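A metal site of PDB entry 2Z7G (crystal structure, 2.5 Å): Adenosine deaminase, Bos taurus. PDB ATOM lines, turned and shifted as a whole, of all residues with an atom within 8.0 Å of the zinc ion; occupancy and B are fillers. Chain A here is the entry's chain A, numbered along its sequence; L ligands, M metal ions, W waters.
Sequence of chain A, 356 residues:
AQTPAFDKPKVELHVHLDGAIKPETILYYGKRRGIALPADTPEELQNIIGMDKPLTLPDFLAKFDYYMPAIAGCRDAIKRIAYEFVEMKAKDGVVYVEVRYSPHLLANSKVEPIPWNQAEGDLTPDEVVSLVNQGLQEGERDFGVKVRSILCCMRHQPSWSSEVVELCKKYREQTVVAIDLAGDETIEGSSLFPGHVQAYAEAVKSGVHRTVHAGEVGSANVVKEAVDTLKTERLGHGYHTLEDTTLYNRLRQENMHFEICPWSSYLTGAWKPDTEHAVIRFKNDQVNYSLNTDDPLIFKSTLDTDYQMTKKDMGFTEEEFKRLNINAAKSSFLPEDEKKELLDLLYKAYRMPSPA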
ATOM      1  N   HIS A  14     -21.322 -18.117  24.382  1.00  0.00           N
ATOM      2  CA  HIS A  14     -22.075 -19.359  24.299  1.00  0.00           C
ATOM      3  C   HIS A  14     -21.577 -20.524  25.173  1.00  0.00           C
ATOM      4  O   HIS A  14     -20.795 -21.364  24.726  1.00  0.00           O
ATOM      5  CB  HIS A  14     -22.175 -19.817  22.832  1.00  0.00           C
ATOM      6  CG  HIS A  14     -23.221 -20.841  22.589  1.00  0.00           C
ATOM      7  ND1 HIS A  14     -24.198 -20.704  21.622  1.00  0.00           N
ATOM      8  CD2 HIS A  14     -23.473 -22.036  23.203  1.00  0.00           C
ATOM      9  CE1 HIS A  14     -24.992 -21.760  21.638  1.00  0.00           C
ATOM     10  NE2 HIS A  14     -24.576 -22.588  22.590  1.00  0.00           N
ATOM     11  N   VAL A  15     -22.073 -20.589  26.405  1.00  0.00           N
ATOM     12  CA  VAL A  15     -21.671 -21.640  27.306  1.00  0.00           C
ATOM     13  C   VAL A  15     -22.793 -21.966  28.299  1.00  0.00           C
ATOM     14  O   VAL A  15     -23.374 -21.079  28.940  1.00  0.00           O
ATOM     15  CB  VAL A  15     -20.361 -21.235  28.037  1.00  0.00           C
ATOM     16  CG1 VAL A  15     -20.610 -20.010  28.942  1.00  0.00           C
ATOM     17  CG2 VAL A  15     -19.803 -22.395  28.830  1.00  0.00           C
ATOM     18  N   HIS A  16     -23.113 -23.266  28.411  1.00  0.00           N
ATOM     19  CA  HIS A  16     -24.165 -23.768  29.318  1.00  0.00           C
ATOM     20  C   HIS A  16     -23.684 -24.000  30.760  1.00  0.00           C
ATOM     21  O   HIS A  16     -22.683 -24.649  30.973  1.00  0.00           O
ATOM     22  CB  HIS A  16     -24.708 -25.099  28.769  1.00  0.00           C
ATOM     23  CG  HIS A  16     -25.314 -24.989  27.424  1.00  0.00           C
ATOM     24  ND1 HIS A  16     -26.665 -24.794  27.210  1.00  0.00           N
ATOM     25  CD2 HIS A  16     -24.764 -25.016  26.180  1.00  0.00           C
ATOM     26  CE1 HIS A  16     -26.929 -24.688  25.919  1.00  0.00           C
ATOM     27  NE2 HIS A  16     -25.772 -24.815  25.275  1.00  0.00           N
ATOM     28  N   PHE A  60     -26.167 -38.802  23.932  1.00  0.00           N
ATOM     29  CA  PHE A  60     -25.763 -37.473  24.396  1.00  0.00           C
ATOM     30  C   PHE A  60     -26.632 -36.935  25.530  1.00  0.00           C
ATOM     31  O   PHE A  60     -26.135 -36.430  26.528  1.00  0.00           O
ATOM     32  CB  PHE A  60     -25.831 -36.482  23.234  1.00  0.00           C
ATOM     33  CG  PHE A  60     -25.533 -35.063  23.648  1.00  0.00           C
ATOM     34  CD1 PHE A  60     -24.236 -34.681  23.963  1.00  0.00           C
ATOM     35  CD2 PHE A  60     -26.556 -34.136  23.762  1.00  0.00           C
ATOM     36  CE1 PHE A  60     -23.976 -33.391  24.378  1.00  0.00           C
ATOM     37  CE2 PHE A  60     -26.295 -32.837  24.177  1.00  0.00           C
ATOM     38  CZ  PHE A  60     -24.998 -32.474  24.493  1.00  0.00           C
ATOM     39  N   ARG A 100     -25.572 -19.493  30.089  1.00  0.00           N
ATOM     40  CA  ARG A 100     -26.977 -19.857  29.892  1.00  0.00           C
ATOM     41  C   ARG A 100     -27.368 -21.220  30.486  1.00  0.00           C
ATOM     42  O   ARG A 100     -26.520 -22.085  30.711  1.00  0.00           O
ATOM     43  CB  ARG A 100     -27.316 -19.860  28.406  1.00  0.00           C
ATOM     44  CG  ARG A 100     -26.569 -20.909  27.603  1.00  0.00           C
ATOM     45  CD  ARG A 100     -26.863 -20.772  26.121  1.00  0.00           C
ATOM     46  NE  ARG A 100     -26.220 -19.604  25.540  1.00  0.00           N
ATOM     47  CZ  ARG A 100     -26.391 -19.207  24.286  1.00  0.00           C
ATOM     48  NH1 ARG A 100     -25.760 -18.142  23.824  1.00  0.00           N
ATOM     49  NH2 ARG A 100     -27.194 -19.866  23.481  1.00  0.00           N
ATOM     50  N   CYS A 152     -32.731 -20.367  28.970  1.00  0.00           N
ATOM     51  CA  CYS A 152     -33.108 -21.114  27.787  1.00  0.00           C
ATOM     52  C   CYS A 152     -34.535 -21.657  27.799  1.00  0.00           C
ATOM     53  O   CYS A 152     -35.067 -22.012  28.843  1.00  0.00           O
ATOM     54  CB  CYS A 152     -32.180 -22.294  27.592  1.00  0.00           C
ATOM     55  SG  CYS A 152     -30.416 -21.869  27.555  1.00  0.00           S
ATOM     56  N   ASP A 180     -33.082 -17.607  25.205  1.00  0.00           N
ATOM     57  CA  ASP A 180     -32.525 -18.512  24.219  1.00  0.00           C
ATOM     58  C   ASP A 180     -33.468 -19.678  23.986  1.00  0.00           C
ATOM     59  O   ASP A 180     -34.428 -19.890  24.738  1.00  0.00           O
ATOM     60  CB  ASP A 180     -31.182 -19.032  24.720  1.00  0.00           C
ATOM     61  CG  ASP A 180     -30.484 -19.941  23.714  1.00  0.00           C
ATOM     62  OD1 ASP A 180     -29.732 -20.842  24.165  1.00  0.00           O
ATOM     63  OD2 ASP A 180     -30.651 -19.782  22.494  1.00  0.00           O
ATOM     64  N   LEU A 181     -33.165 -20.432  22.933  1.00  0.00           N
ATOM     65  CA  LEU A 181     -33.931 -21.599  22.549  1.00  0.00           C
ATOM     66  C   LEU A 181     -32.890 -22.704  22.302  1.00  0.00           C
ATOM     67  O   LEU A 181     -32.037 -22.578  21.418  1.00  0.00           O
ATOM     68  CB  LEU A 181     -34.702 -21.334  21.247  1.00  0.00           C
ATOM     69  CG  LEU A 181     -36.123 -21.916  21.091  1.00  0.00           C
ATOM     70  CD1 LEU A 181     -36.417 -22.120  19.620  1.00  0.00           C
ATOM     71  CD2 LEU A 181     -36.252 -23.226  21.825  1.00  0.00           C
ATOM     72  N   ALA A 182     -32.955 -23.773  23.078  1.00  0.00           N
ATOM     73  CA  ALA A 182     -32.002 -24.862  22.912  1.00  0.00           C
ATOM     74  C   ALA A 182     -32.801 -26.156  22.778  1.00  0.00           C
ATOM     75  O   ALA A 182     -34.013 -26.137  22.892  1.00  0.00           O
ATOM     76  CB  ALA A 182     -31.076 -24.936  24.112  1.00  0.00           C
ATOM     77  N   GLY A 183     -32.108 -27.275  22.527  1.00  0.00           N
ATOM     78  CA  GLY A 183     -32.816 -28.542  22.365  1.00  0.00           C
ATOM     79  C   GLY A 183     -32.824 -29.098  20.949  1.00  0.00           C
ATOM     80  O   GLY A 183     -32.316 -28.467  20.012  1.00  0.00           O
ATOM     81  N   HIS A 213     -30.457 -21.258  19.323  1.00  0.00           N
ATOM     82  CA  HIS A 213     -29.568 -22.323  18.840  1.00  0.00           C
ATOM     83  C   HIS A 213     -30.200 -22.772  17.512  1.00  0.00           C
ATOM     84  O   HIS A 213     -31.247 -23.403  17.510  1.00  0.00           O
ATOM     85  CB  HIS A 213     -29.579 -23.544  19.784  1.00  0.00           C
ATOM     86  CG  HIS A 213     -28.657 -23.428  20.967  1.00  0.00           C
ATOM     87  ND1 HIS A 213     -28.956 -22.672  22.076  1.00  0.00           N
ATOM     88  CD2 HIS A 213     -27.483 -24.048  21.227  1.00  0.00           C
ATOM     89  CE1 HIS A 213     -28.004 -22.822  22.981  1.00  0.00           C
ATOM     90  NE2 HIS A 213     -27.103 -23.647  22.491  1.00  0.00           N
ATOM     91  N   GLU A 216     -27.033 -25.670  13.925  1.00  0.00           N
ATOM     92  CA  GLU A 216     -26.037 -26.593  14.436  1.00  0.00           C
ATOM     93  C   GLU A 216     -26.192 -27.949  13.742  1.00  0.00           C
ATOM     94  O   GLU A 216     -25.222 -28.535  13.258  1.00  0.00           O
ATOM     95  CB  GLU A 216     -26.181 -26.758  15.969  1.00  0.00           C
ATOM     96  CG  GLU A 216     -25.321 -27.865  16.560  1.00  0.00           C
ATOM     97  CD  GLU A 216     -25.371 -27.932  18.090  1.00  0.00           C
ATOM     98  OE1 GLU A 216     -26.482 -27.880  18.672  1.00  0.00           O
ATOM     99  OE2 GLU A 216     -24.304 -28.080  18.705  1.00  0.00           O
ATOM    100  N   GLY A 236     -26.889 -19.265  17.798  1.00  0.00           N
ATOM    101  CA  GLY A 236     -26.050 -20.227  18.468  1.00  0.00           C
ATOM    102  C   GLY A 236     -25.626 -21.234  17.395  1.00  0.00           C
ATOM    103  O   GLY A 236     -26.460 -21.977  16.879  1.00  0.00           O
ATOM    104  N   HIS A 237     -24.347 -21.218  17.027  1.00  0.00           N
ATOM    105  CA  HIS A 237     -23.842 -22.114  15.994  1.00  0.00           C
ATOM    106  C   HIS A 237     -24.116 -21.584  14.583  1.00  0.00           C
ATOM    107  O   HIS A 237     -23.246 -20.962  13.976  1.00  0.00           O
ATOM    108  CB  HIS A 237     -24.474 -23.507  16.140  1.00  0.00           C
ATOM    109  CG  HIS A 237     -24.166 -24.175  17.430  1.00  0.00           C
ATOM    110  ND1 HIS A 237     -22.889 -24.520  17.805  1.00  0.00           N
ATOM    111  CD2 HIS A 237     -24.971 -24.596  18.434  1.00  0.00           C
ATOM    112  CE1 HIS A 237     -22.924 -25.117  18.979  1.00  0.00           C
ATOM    113  NE2 HIS A 237     -24.181 -25.181  19.383  1.00  0.00           N
ATOM    114  N   GLU A 259     -22.452 -17.527  17.231  1.00  0.00           N
ATOM    115  CA  GLU A 259     -21.798 -18.046  18.432  1.00  0.00           C
ATOM    116  C   GLU A 259     -21.230 -19.400  18.043  1.00  0.00           C
ATOM    117  O   GLU A 259     -21.906 -20.424  18.137  1.00  0.00           O
ATOM    118  CB  GLU A 259     -22.832 -18.187  19.545  1.00  0.00           C
ATOM    119  CG  GLU A 259     -23.509 -16.874  19.892  1.00  0.00           C
ATOM    120  CD  GLU A 259     -24.778 -17.056  20.700  1.00  0.00           C
ATOM    121  OE1 GLU A 259     -25.106 -18.214  21.039  1.00  0.00           O
ATOM    122  OE2 GLU A 259     -25.437 -16.047  20.976  1.00  0.00           O
ATOM    123  N   CYS A 261     -18.838 -22.773  18.212  1.00  0.00           N
ATOM    124  CA  CYS A 261     -18.275 -23.724  19.171  1.00  0.00           C
ATOM    125  C   CYS A 261     -17.514 -24.801  18.397  1.00  0.00           C
ATOM    126  O   CYS A 261     -17.992 -25.923  18.231  1.00  0.00           O
ATOM    127  CB  CYS A 261     -19.405 -24.359  19.989  1.00  0.00           C
ATOM    128  SG  CYS A 261     -20.585 -23.167  20.699  1.00  0.00           S
ATOM    129  N   SER A 264     -16.785 -28.160  20.098  1.00  0.00           N
ATOM    130  CA  SER A 264     -18.119 -28.715  20.291  1.00  0.00           C
ATOM    131  C   SER A 264     -18.674 -29.353  19.019  1.00  0.00           C
ATOM    132  O   SER A 264     -19.171 -30.484  19.053  1.00  0.00           O
ATOM    133  CB  SER A 264     -19.079 -27.639  20.763  1.00  0.00           C
ATOM    134  OG  SER A 264     -20.401 -28.136  20.732  1.00  0.00           O
ATOM    135  N   ASN A 292     -16.609 -20.134  21.326  1.00  0.00           N
ATOM    136  CA  ASN A 292     -17.166 -20.545  22.622  1.00  0.00           C
ATOM    137  C   ASN A 292     -16.915 -22.026  22.929  1.00  0.00           C
ATOM    138  O   ASN A 292     -16.670 -22.820  22.031  1.00  0.00           O
ATOM    139  CB  ASN A 292     -18.669 -20.257  22.601  1.00  0.00           C
ATOM    140  CG  ASN A 292     -18.985 -18.796  22.277  1.00  0.00           C
ATOM    141  OD1 ASN A 292     -19.195 -17.993  23.167  1.00  0.00           O
ATOM    142  ND2 ASN A 292     -18.989 -18.454  20.991  1.00  0.00           N
ATOM    143  N   THR A 293     -16.982 -22.376  24.220  1.00  0.00           N
ATOM    144  CA  THR A 293     -16.758 -23.749  24.657  1.00  0.00           C
ATOM    145  C   THR A 293     -18.031 -24.588  24.628  1.00  0.00           C
ATOM    146  O   THR A 293     -17.984 -25.795  24.363  1.00  0.00           O
ATOM    147  CB  THR A 293     -16.160 -23.823  26.100  1.00  0.00           C
ATOM    148  OG1 THR A 293     -17.059 -23.206  27.025  1.00  0.00           O
ATOM    149  CG2 THR A 293     -14.818 -23.125  26.161  1.00  0.00           C
ATOM    150  N   ASP A 294     -19.164 -23.959  24.933  1.00  0.00           N
ATOM    151  CA  ASP A 294     -20.466 -24.634  24.946  1.00  0.00           C
ATOM    152  C   ASP A 294     -20.681 -25.484  26.206  1.00  0.00           C
ATOM    153  O   ASP A 294     -21.519 -25.152  27.044  1.00  0.00           O
ATOM    154  CB  ASP A 294     -20.595 -25.501  23.672  1.00  0.00           C
ATOM    155  CG  ASP A 294     -22.042 -25.706  23.249  1.00  0.00           C
ATOM    156  OD1 ASP A 294     -22.970 -25.124  23.880  1.00  0.00           O
ATOM    157  OD2 ASP A 294     -22.253 -26.466  22.272  1.00  0.00           O
ATOM    158  N   ASP A 295     -19.911 -26.563  26.347  1.00  0.00           N
ATOM    159  CA  ASP A 295     -20.025 -27.450  27.512  1.00  0.00           C
ATOM    160  C   ASP A 295     -18.662 -28.038  27.860  1.00  0.00           C
ATOM    161  O   ASP A 295     -18.317 -29.130  27.412  1.00  0.00           O
ATOM    162  CB  ASP A 295     -20.990 -28.597  27.243  1.00  0.00           C
ATOM    163  CG  ASP A 295     -22.347 -28.116  26.773  1.00  0.00           C
ATOM    164  OD1 ASP A 295     -23.314 -28.104  27.584  1.00  0.00           O
ATOM    165  OD2 ASP A 295     -22.444 -27.737  25.588  1.00  0.00           O
ATOM    166  N   PHE A 299     -17.387 -31.964  26.822  1.00  0.00           N
ATOM    167  CA  PHE A 299     -16.314 -31.968  25.834  1.00  0.00           C
ATOM    168  C   PHE A 299     -14.918 -31.951  26.454  1.00  0.00           C
ATOM    169  O   PHE A 299     -13.921 -31.768  25.751  1.00  0.00           O
ATOM    170  CB  PHE A 299     -16.490 -30.784  24.873  1.00  0.00           C
ATOM    171  CG  PHE A 299     -17.868 -30.679  24.275  1.00  0.00           C
ATOM    172  CD1 PHE A 299     -18.458 -31.783  23.666  1.00  0.00           C
ATOM    173  CD2 PHE A 299     -18.609 -29.508  24.383  1.00  0.00           C
ATOM    174  CE1 PHE A 299     -19.736 -31.697  23.121  1.00  0.00           C
ATOM    175  CE2 PHE A 299     -19.886 -29.422  23.838  1.00  0.00           C
ATOM    176  CZ  PHE A 299     -20.455 -30.525  23.236  1.00  0.00           C
HETATM  177  C1  LIG L   1     -26.596 -28.531  24.234  1.00  0.00           C
HETATM  178  C2  LIG L   1     -26.662 -28.297  25.579  1.00  0.00           C
HETATM  179  C3  LIG L   1     -27.913 -28.210  26.195  1.00  0.00           C
HETATM  180  C4  LIG L   1     -28.991 -28.586  24.211  1.00  0.00           C
HETATM  181  C5  LIG L   1     -26.323 -27.971  27.680  1.00  0.00           C
HETATM  182  N1  LIG L   1     -29.101 -28.353  25.530  1.00  0.00           N
HETATM  183  N2  LIG L   1     -27.799 -28.674  23.570  1.00  0.00           N
HETATM  184  N3  LIG L   1     -27.668 -27.973  27.525  1.00  0.00           N
HETATM  185  N4  LIG L   1     -25.717 -28.127  26.482  1.00  0.00           N
HETATM  186  C6  LIG L   1     -28.521 -27.773  28.711  1.00  0.00           C
HETATM  187  C7  LIG L   1     -29.247 -29.044  29.224  1.00  0.00           C
HETATM  188  N5  LIG L   1     -25.441 -28.630  23.546  1.00  0.00           N
HETATM  189  C8  LIG L   1     -30.159 -29.703  28.197  1.00  0.00           C
HETATM  190  C9  LIG L   1     -30.864 -30.992  28.554  1.00  0.00           C
HETATM  191  C10 LIG L   1     -31.483 -31.531  27.244  1.00  0.00           C
HETATM  192  C11 LIG L   1     -30.497 -31.484  26.052  1.00  0.00           C
HETATM  193  C12 LIG L   1     -30.466 -32.752  25.196  1.00  0.00           C
HETATM  194  C13 LIG L   1     -29.283 -26.454  28.763  1.00  0.00           C
HETATM  195  O1  LIG L   1     -28.367 -25.410  28.940  1.00  0.00           O
HETATM  196  C14 LIG L   1     -30.442 -26.203  27.799  1.00  0.00           C
HETATM  197 ZN    ZN M   1     -25.157 -24.646  23.223  1.00  0.00          ZN
HETATM  198  O   HOH W   1     -24.656 -26.197  21.948  1.00  0.00           O
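NE2 of His 237 touches the zinc ion, at 3.998 Å.
Five residues have an atom within 4 Å of the zinc ion: His 14, His 16, His 213, His 237 and Asp 294.
The nearest printed residue that does not touch the zinc ion is Asp 295 (4.7 Å).
Water W1 lies within hydrogen-bond range of OD2 of Asp 294 (2.4 Å), NE2 of His 237 (2.8 Å) and N5 of the ligand (3.0 Å).
ND1 of His 14 lies within hydrogen-bond range of OE1 of Glu 259.
The backbone NH of His 14 lies within hydrogen-bond range of the side-chain amide oxygen of Asn 292 (2.5 Å).
OD1 of Asp 180 lies close to ND1 of His 213 (2.9 Å).
N of His 213 lies within hydrogen-bond range of O of Leu 181, at 2.9 Å.
OD2 of Asp 294 lies within hydrogen-bond range of OG of Ser 264 (2.9 Å).
The side-chain carboxylate (OE2) of Glu 216 is in hydrogen-bond range of a ring nitrogen (NE2) of His 237, at 3.0 Å.
The backbone carbonyl oxygen of Glu 259 lies within hydrogen-bond range of the backbone NH of His 237, 2.8 Å away.
Water W1 binds the zinc ion.
NE2 of His 16 binds the zinc ion (2.1 Å).
The zinc ion is bound by NE2 of His 14 (2.2 Å).
The zinc ion is bound by NE2 of His 213, at 2.3 Å.
OD1 of Asp 294 is bound to the zinc ion, 2.3 Å away.
The zinc ion has five donor atoms within binding distance.
O1 of the ligand is in hydrogen-bond range of ND1 of His 16 (2.5 Å).
The side-chain carboxylate (OD1) of Asp 295 lies within hydrogen-bond range of a nitrogen (N4) of the ligand (2.6 Å).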
